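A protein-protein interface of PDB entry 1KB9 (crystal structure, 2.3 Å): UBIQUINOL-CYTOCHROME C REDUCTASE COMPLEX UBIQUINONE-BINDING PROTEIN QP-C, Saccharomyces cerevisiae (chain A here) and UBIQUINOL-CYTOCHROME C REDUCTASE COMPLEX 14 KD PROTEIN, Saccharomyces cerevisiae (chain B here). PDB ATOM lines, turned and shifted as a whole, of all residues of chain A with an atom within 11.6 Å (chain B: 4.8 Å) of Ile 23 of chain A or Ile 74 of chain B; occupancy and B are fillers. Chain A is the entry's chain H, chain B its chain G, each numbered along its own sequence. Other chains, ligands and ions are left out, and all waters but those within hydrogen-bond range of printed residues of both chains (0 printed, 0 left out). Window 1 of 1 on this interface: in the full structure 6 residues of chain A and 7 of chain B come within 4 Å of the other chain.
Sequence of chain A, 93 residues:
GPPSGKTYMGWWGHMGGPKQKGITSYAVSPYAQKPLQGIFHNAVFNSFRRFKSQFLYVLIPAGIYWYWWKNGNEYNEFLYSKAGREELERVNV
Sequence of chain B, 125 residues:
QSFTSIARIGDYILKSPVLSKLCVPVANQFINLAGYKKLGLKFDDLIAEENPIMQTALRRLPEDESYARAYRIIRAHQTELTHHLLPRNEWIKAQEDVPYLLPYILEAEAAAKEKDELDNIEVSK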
ATOM      1  N   MET A  15     -10.011  17.414  15.909  1.00  0.00           N
ATOM      2  CA  MET A  15      -9.250  17.674  14.693  1.00  0.00           C
ATOM      3  C   MET A  15      -9.746  16.934  13.467  1.00  0.00           C
ATOM      4  O   MET A  15      -9.534  17.389  12.340  1.00  0.00           O
ATOM      5  CB  MET A  15      -7.768  17.376  14.906  1.00  0.00           C
ATOM      6  CG  MET A  15      -6.846  18.252  14.073  1.00  0.00           C
ATOM      7  SD  MET A  15      -6.983  19.998  14.518  1.00  0.00           S
ATOM      8  CE  MET A  15      -6.051  20.030  16.050  1.00  0.00           C
ATOM      9  N   GLY A  16     -10.404  15.798  13.691  1.00  0.00           N
ATOM     10  CA  GLY A  16     -10.924  15.015  12.586  1.00  0.00           C
ATOM     11  C   GLY A  16     -10.072  13.804  12.238  1.00  0.00           C
ATOM     12  O   GLY A  16     -10.340  13.112  11.253  1.00  0.00           O
ATOM     13  N   GLY A  17      -9.020  13.571  13.018  1.00  0.00           N
ATOM     14  CA  GLY A  17      -8.168  12.425  12.783  1.00  0.00           C
ATOM     15  C   GLY A  17      -8.804  11.174  13.359  1.00  0.00           C
ATOM     16  O   GLY A  17      -9.895  11.241  13.938  1.00  0.00           O
ATOM     17  N   PRO A  18      -8.166  10.006  13.192  1.00  0.00           N
ATOM     18  CA  PRO A  18      -8.714   8.754  13.724  1.00  0.00           C
ATOM     19  C   PRO A  18      -8.439   8.703  15.226  1.00  0.00           C
ATOM     20  O   PRO A  18      -7.564   9.424  15.719  1.00  0.00           O
ATOM     21  CB  PRO A  18      -7.900   7.696  12.977  1.00  0.00           C
ATOM     22  CG  PRO A  18      -6.539   8.335  12.899  1.00  0.00           C
ATOM     23  CD  PRO A  18      -6.899   9.763  12.476  1.00  0.00           C
ATOM     24  N   LYS A  19      -9.171   7.856  15.946  1.00  0.00           N
ATOM     25  CA  LYS A  19      -8.974   7.725  17.388  1.00  0.00           C
ATOM     26  C   LYS A  19      -7.599   7.136  17.692  1.00  0.00           C
ATOM     27  O   LYS A  19      -7.248   6.085  17.184  1.00  0.00           O
ATOM     28  CB  LYS A  19     -10.077   6.865  18.007  1.00  0.00           C
ATOM     29  CG  LYS A  19     -11.476   7.391  17.735  1.00  0.00           C
ATOM     30  CD  LYS A  19     -12.471   6.957  18.792  1.00  0.00           C
ATOM     31  CE  LYS A  19     -13.907   7.290  18.368  1.00  0.00           C
ATOM     32  NZ  LYS A  19     -14.076   8.710  17.896  1.00  0.00           N
ATOM     33  N   GLN A  20      -6.811   7.842  18.489  1.00  0.00           N
ATOM     34  CA  GLN A  20      -5.468   7.392  18.837  1.00  0.00           C
ATOM     35  C   GLN A  20      -5.449   6.647  20.158  1.00  0.00           C
ATOM     36  O   GLN A  20      -6.090   7.059  21.121  1.00  0.00           O
ATOM     37  CB  GLN A  20      -4.505   8.582  18.908  1.00  0.00           C
ATOM     38  CG  GLN A  20      -4.327   9.331  17.599  1.00  0.00           C
ATOM     39  CD  GLN A  20      -3.353  10.484  17.726  1.00  0.00           C
ATOM     40  OE1 GLN A  20      -2.473  10.469  18.586  1.00  0.00           O
ATOM     41  NE2 GLN A  20      -3.505  11.493  16.874  1.00  0.00           N
ATOM     42  N   LYS A  21      -4.687   5.559  20.204  1.00  0.00           N
ATOM     43  CA  LYS A  21      -4.563   4.738  21.404  1.00  0.00           C
ATOM     44  C   LYS A  21      -3.252   3.963  21.308  1.00  0.00           C
ATOM     45  O   LYS A  21      -2.879   3.511  20.228  1.00  0.00           O
ATOM     46  CB  LYS A  21      -5.736   3.761  21.484  1.00  0.00           C
ATOM     47  CG  LYS A  21      -5.874   3.026  22.812  1.00  0.00           C
ATOM     48  CD  LYS A  21      -7.024   2.010  22.747  1.00  0.00           C
ATOM     49  CE  LYS A  21      -7.535   1.614  24.132  1.00  0.00           C
ATOM     50  NZ  LYS A  21      -6.462   1.084  25.004  1.00  0.00           N
ATOM     51  N   GLY A  22      -2.535   3.855  22.423  1.00  0.00           N
ATOM     52  CA  GLY A  22      -1.285   3.119  22.433  1.00  0.00           C
ATOM     53  C   GLY A  22      -0.016   3.913  22.192  1.00  0.00           C
ATOM     54  O   GLY A  22       1.086   3.417  22.439  1.00  0.00           O
ATOM     55  N   ILE A  23      -0.158   5.132  21.681  1.00  0.00           N
ATOM     56  CA  ILE A  23       0.995   5.990  21.408  1.00  0.00           C
ATOM     57  C   ILE A  23       1.241   6.890  22.617  1.00  0.00           C
ATOM     58  O   ILE A  23       0.329   7.563  23.092  1.00  0.00           O
ATOM     59  CB  ILE A  23       0.738   6.876  20.173  1.00  0.00           C
ATOM     60  CG1 ILE A  23       0.335   6.005  18.980  1.00  0.00           C
ATOM     61  CG2 ILE A  23       1.973   7.722  19.864  1.00  0.00           C
ATOM     62  CD1 ILE A  23      -0.271   6.768  17.826  1.00  0.00           C
ATOM     63  N   THR A  24       2.475   6.896  23.105  1.00  0.00           N
ATOM     64  CA  THR A  24       2.863   7.703  24.250  1.00  0.00           C
ATOM     65  C   THR A  24       4.017   8.600  23.814  1.00  0.00           C
ATOM     66  O   THR A  24       4.982   8.121  23.221  1.00  0.00           O
ATOM     67  CB  THR A  24       3.319   6.785  25.429  1.00  0.00           C
ATOM     68  OG1 THR A  24       2.212   5.987  25.859  1.00  0.00           O
ATOM     69  CG2 THR A  24       3.836   7.595  26.612  1.00  0.00           C
ATOM     70  N   SER A  25       3.924   9.900  24.086  1.00  0.00           N
ATOM     71  CA  SER A  25       4.996  10.806  23.688  1.00  0.00           C
ATOM     72  C   SER A  25       5.712  11.396  24.881  1.00  0.00           C
ATOM     73  O   SER A  25       5.142  11.523  25.961  1.00  0.00           O
ATOM     74  CB  SER A  25       4.474  11.925  22.772  1.00  0.00           C
ATOM     75  OG  SER A  25       3.561  12.780  23.440  1.00  0.00           O
ATOM     76  N   TYR A  26       6.971  11.752  24.682  1.00  0.00           N
ATOM     77  CA  TYR A  26       7.775  12.327  25.750  1.00  0.00           C
ATOM     78  C   TYR A  26       8.516  13.527  25.204  1.00  0.00           C
ATOM     79  O   TYR A  26       8.919  13.530  24.040  1.00  0.00           O
ATOM     80  CB  TYR A  26       8.819  11.318  26.248  1.00  0.00           C
ATOM     81  CG  TYR A  26       8.265  10.006  26.756  1.00  0.00           C
ATOM     82  CD1 TYR A  26       7.917   8.985  25.871  1.00  0.00           C
ATOM     83  CD2 TYR A  26       8.141   9.762  28.127  1.00  0.00           C
ATOM     84  CE1 TYR A  26       7.465   7.757  26.336  1.00  0.00           C
ATOM     85  CE2 TYR A  26       7.696   8.531  28.602  1.00  0.00           C
ATOM     86  CZ  TYR A  26       7.361   7.534  27.704  1.00  0.00           C
ATOM     87  OH  TYR A  26       6.938   6.307  28.166  1.00  0.00           O
ATOM     88  N   ALA A  27       8.729  14.527  26.052  1.00  0.00           N
ATOM     89  CA  ALA A  27       9.455  15.716  25.645  1.00  0.00           C
ATOM     90  C   ALA A  27      10.124  16.342  26.866  1.00  0.00           C
ATOM     91  O   ALA A  27       9.721  16.094  28.001  1.00  0.00           O
ATOM     92  CB  ALA A  27       8.510  16.723  24.959  1.00  0.00           C
ATOM     93  N   TYR B  67      -4.892   1.908  14.586  1.00  0.00           N
ATOM     94  CA  TYR B  67      -3.956   2.464  15.562  1.00  0.00           C
ATOM     95  C   TYR B  67      -2.539   2.412  15.003  1.00  0.00           C
ATOM     96  O   TYR B  67      -1.728   3.302  15.267  1.00  0.00           O
ATOM     97  CB  TYR B  67      -4.005   1.691  16.889  1.00  0.00           C
ATOM     98  CG  TYR B  67      -5.347   1.698  17.599  1.00  0.00           C
ATOM     99  CD1 TYR B  67      -5.807   0.557  18.260  1.00  0.00           C
ATOM    100  CD2 TYR B  67      -6.153   2.843  17.621  1.00  0.00           C
ATOM    101  CE1 TYR B  67      -7.028   0.555  18.923  1.00  0.00           C
ATOM    102  CE2 TYR B  67      -7.376   2.849  18.279  1.00  0.00           C
ATOM    103  CZ  TYR B  67      -7.807   1.702  18.928  1.00  0.00           C
ATOM    104  OH  TYR B  67      -9.017   1.697  19.588  1.00  0.00           O
ATOM    105  N   ALA B  70      -1.941   5.141  12.453  1.00  0.00           N
ATOM    106  CA  ALA B  70      -1.788   6.387  13.208  1.00  0.00           C
ATOM    107  C   ALA B  70      -0.365   6.581  13.721  1.00  0.00           C
ATOM    108  O   ALA B  70       0.201   7.675  13.611  1.00  0.00           O
ATOM    109  CB  ALA B  70      -2.783   6.435  14.369  1.00  0.00           C
ATOM    110  N   TYR B  71       0.209   5.520  14.278  1.00  0.00           N
ATOM    111  CA  TYR B  71       1.574   5.588  14.790  1.00  0.00           C
ATOM    112  C   TYR B  71       2.583   5.819  13.670  1.00  0.00           C
ATOM    113  O   TYR B  71       3.505   6.621  13.819  1.00  0.00           O
ATOM    114  CB  TYR B  71       1.946   4.310  15.561  1.00  0.00           C
ATOM    115  CG  TYR B  71       3.382   4.310  16.028  1.00  0.00           C
ATOM    116  CD1 TYR B  71       3.848   5.298  16.892  1.00  0.00           C
ATOM    117  CD2 TYR B  71       4.295   3.371  15.548  1.00  0.00           C
ATOM    118  CE1 TYR B  71       5.190   5.359  17.262  1.00  0.00           C
ATOM    119  CE2 TYR B  71       5.646   3.423  15.913  1.00  0.00           C
ATOM    120  CZ  TYR B  71       6.084   4.422  16.769  1.00  0.00           C
ATOM    121  OH  TYR B  71       7.416   4.502  17.121  1.00  0.00           O
ATOM    122  N   ARG B  72       2.415   5.107  12.557  1.00  0.00           N
ATOM    123  CA  ARG B  72       3.330   5.247  11.429  1.00  0.00           C
ATOM    124  C   ARG B  72       3.316   6.663  10.866  1.00  0.00           C
ATOM    125  O   ARG B  72       4.374   7.244  10.603  1.00  0.00           O
ATOM    126  CB  ARG B  72       3.019   4.222  10.328  1.00  0.00           C
ATOM    127  CG  ARG B  72       3.295   2.778  10.725  1.00  0.00           C
ATOM    128  CD  ARG B  72       3.360   1.860   9.510  1.00  0.00           C
ATOM    129  NE  ARG B  72       2.108   1.830   8.756  1.00  0.00           N
ATOM    130  CZ  ARG B  72       1.074   1.043   9.036  1.00  0.00           C
ATOM    131  NH1 ARG B  72      -0.022   1.097   8.290  1.00  0.00           N
ATOM    132  NH2 ARG B  72       1.137   0.200  10.054  1.00  0.00           N
ATOM    133  N   ILE B  73       2.119   7.226  10.725  1.00  0.00           N
ATOM    134  CA  ILE B  73       1.954   8.586  10.214  1.00  0.00           C
ATOM    135  C   ILE B  73       2.578   9.623  11.164  1.00  0.00           C
ATOM    136  O   ILE B  73       3.329  10.509  10.734  1.00  0.00           O
ATOM    137  CB  ILE B  73       0.468   8.889   9.953  1.00  0.00           C
ATOM    138  CG1 ILE B  73      -0.011   8.060   8.754  1.00  0.00           C
ATOM    139  CG2 ILE B  73       0.252  10.390   9.712  1.00  0.00           C
ATOM    140  CD1 ILE B  73      -1.506   8.094   8.527  1.00  0.00           C
ATOM    141  N   ILE B  74       2.311   9.480  12.458  1.00  0.00           N
ATOM    142  CA  ILE B  74       2.875  10.407  13.433  1.00  0.00           C
ATOM    143  C   ILE B  74       4.395  10.287  13.457  1.00  0.00           C
ATOM    144  O   ILE B  74       5.105  11.293  13.434  1.00  0.00           O
ATOM    145  CB  ILE B  74       2.296  10.185  14.845  1.00  0.00           C
ATOM    146  CG1 ILE B  74       0.807  10.529  14.852  1.00  0.00           C
ATOM    147  CG2 ILE B  74       3.020  11.050  15.854  1.00  0.00           C
ATOM    148  CD1 ILE B  74       0.104  10.201  16.145  1.00  0.00           C
ATOM    149  N   ARG B  75       4.892   9.057  13.444  1.00  0.00           N
ATOM    150  CA  ARG B  75       6.338   8.816  13.457  1.00  0.00           C
ATOM    151  C   ARG B  75       7.005   9.414  12.210  1.00  0.00           C
ATOM    152  O   ARG B  75       8.104   9.961  12.285  1.00  0.00           O
ATOM    153  CB  ARG B  75       6.620   7.313  13.564  1.00  0.00           C
ATOM    154  CG  ARG B  75       8.084   6.941  13.659  1.00  0.00           C
ATOM    155  CD  ARG B  75       8.382   5.790  12.709  1.00  0.00           C
ATOM    156  NE  ARG B  75       8.293   4.465  13.319  1.00  0.00           N
ATOM    157  CZ  ARG B  75       7.823   3.377  12.713  1.00  0.00           C
ATOM    158  NH1 ARG B  75       7.815   2.225  13.364  1.00  0.00           N
ATOM    159  NH2 ARG B  75       7.308   3.439  11.494  1.00  0.00           N
ATOM    160  N   ALA B  76       6.318   9.342  11.072  1.00  0.00           N
ATOM    161  CA  ALA B  76       6.851   9.901   9.831  1.00  0.00           C
ATOM    162  C   ALA B  76       6.967  11.436   9.897  1.00  0.00           C
ATOM    163  O   ALA B  76       7.973  12.005   9.449  1.00  0.00           O
ATOM    164  CB  ALA B  76       5.990   9.476   8.639  1.00  0.00           C
ATOM    165  N   HIS B  77       5.954  12.105  10.455  1.00  0.00           N
ATOM    166  CA  HIS B  77       5.992  13.564  10.568  1.00  0.00           C
ATOM    167  C   HIS B  77       7.130  14.037  11.463  1.00  0.00           C
ATOM    168  O   HIS B  77       7.836  14.993  11.120  1.00  0.00           O
ATOM    169  CB  HIS B  77       4.657  14.127  11.067  1.00  0.00           C
ATOM    170  CG  HIS B  77       3.610  14.237  10.000  1.00  0.00           C
ATOM    171  ND1 HIS B  77       2.467  13.466   9.993  1.00  0.00           N
ATOM    172  CD2 HIS B  77       3.528  15.040   8.913  1.00  0.00           C
ATOM    173  CE1 HIS B  77       1.724  13.793   8.950  1.00  0.00           C
ATOM    174  NE2 HIS B  77       2.345  14.747   8.280  1.00  0.00           N
ATOM    175  N   GLN B  78       7.315  13.355  12.593  1.00  0.00           N
ATOM    176  CA  GLN B  78       8.377  13.701  13.536  1.00  0.00           C
ATOM    177  C   GLN B  78       9.759  13.513  12.917  1.00  0.00           C
ATOM    178  O   GLN B  78      10.640  14.360  13.076  1.00  0.00           O
ATOM    179  CB  GLN B  78       8.263  12.862  14.807  1.00  0.00           C
ATOM    180  CG  GLN B  78       9.357  13.147  15.824  1.00  0.00           C
ATOM    181  CD  GLN B  78       9.306  14.564  16.368  1.00  0.00           C
ATOM    182  OE1 GLN B  78       8.232  15.153  16.505  1.00  0.00           O
ATOM    183  NE2 GLN B  78      10.467  15.117  16.685  1.00  0.00           N
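Of the printed residues of chain B, Lys 21 of chain A touches Tyr 67 (3.7 Å).
Of chain B, only Tyr 71 (3.7 Å) and Ile 74 (3.8 Å) come within 4 Å of Ile 23 of chain A.
Ser 25 of chain A touches none of the printed residues of chain B.
Of the printed residues of chain A, Tyr 67 of chain B touches Lys 19 and Lys 21.
Printed residues of chain A within 4 Å of Tyr 71 of chain B: Ile 23.
No residue of chain A comes within 4 Å of Ile 73 of chain B.
Of chain A, only Gln 20 (3.6 Å) and Ile 23 (3.8 Å) come within 4 Å of Ile 74 of chain B.
No residue of chain A comes within 4 Å of Ala 76 of chain B.
No residue of chain A comes within 4 Å of His 77 of chain B.
No residue of chain A comes within 4 Å of Gln 78 of chain B.
The nearest residue of chain A that does not touch Ile 74 of chain B is Ser 25 of chain A (7.1 Å).
The nearest printed residue of chain B that does not touch Lys 19 of chain A is Ala 70 of chain B (5.3 Å).
Among the printed residues, merely in contact across the chains: Lys 19 of chain A with Tyr 67 of chain B (3.4 Å), Gln 20 of chain A with Ile 74 of chain B (3.6 Å), Lys 21 of chain A with Tyr 67 of chain B (3.7 Å), Ile 23 of chain A with Tyr 71 of chain B (3.7 Å) and Ile 23 of chain A with Ile 74 of chain B (3.8 Å).
Of the 13 printed residues of chain A, 4 touch a printed residue of chain B.
Printed residues of chain A that touch a printed residue of chain B: Lys 19, Gln 20, Lys 21 and Ile 23.
Hydrophobic or aromatic side chains of chain A within 4 Å of the printed part of chain B: Ile 23.
Of the 10 printed residues of chain B, 3 touch a printed residue of chain A.
Hydrophobic or aromatic side chains of chain B within 4 Å of the printed part of chain A: Tyr 67 and Ile 74.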
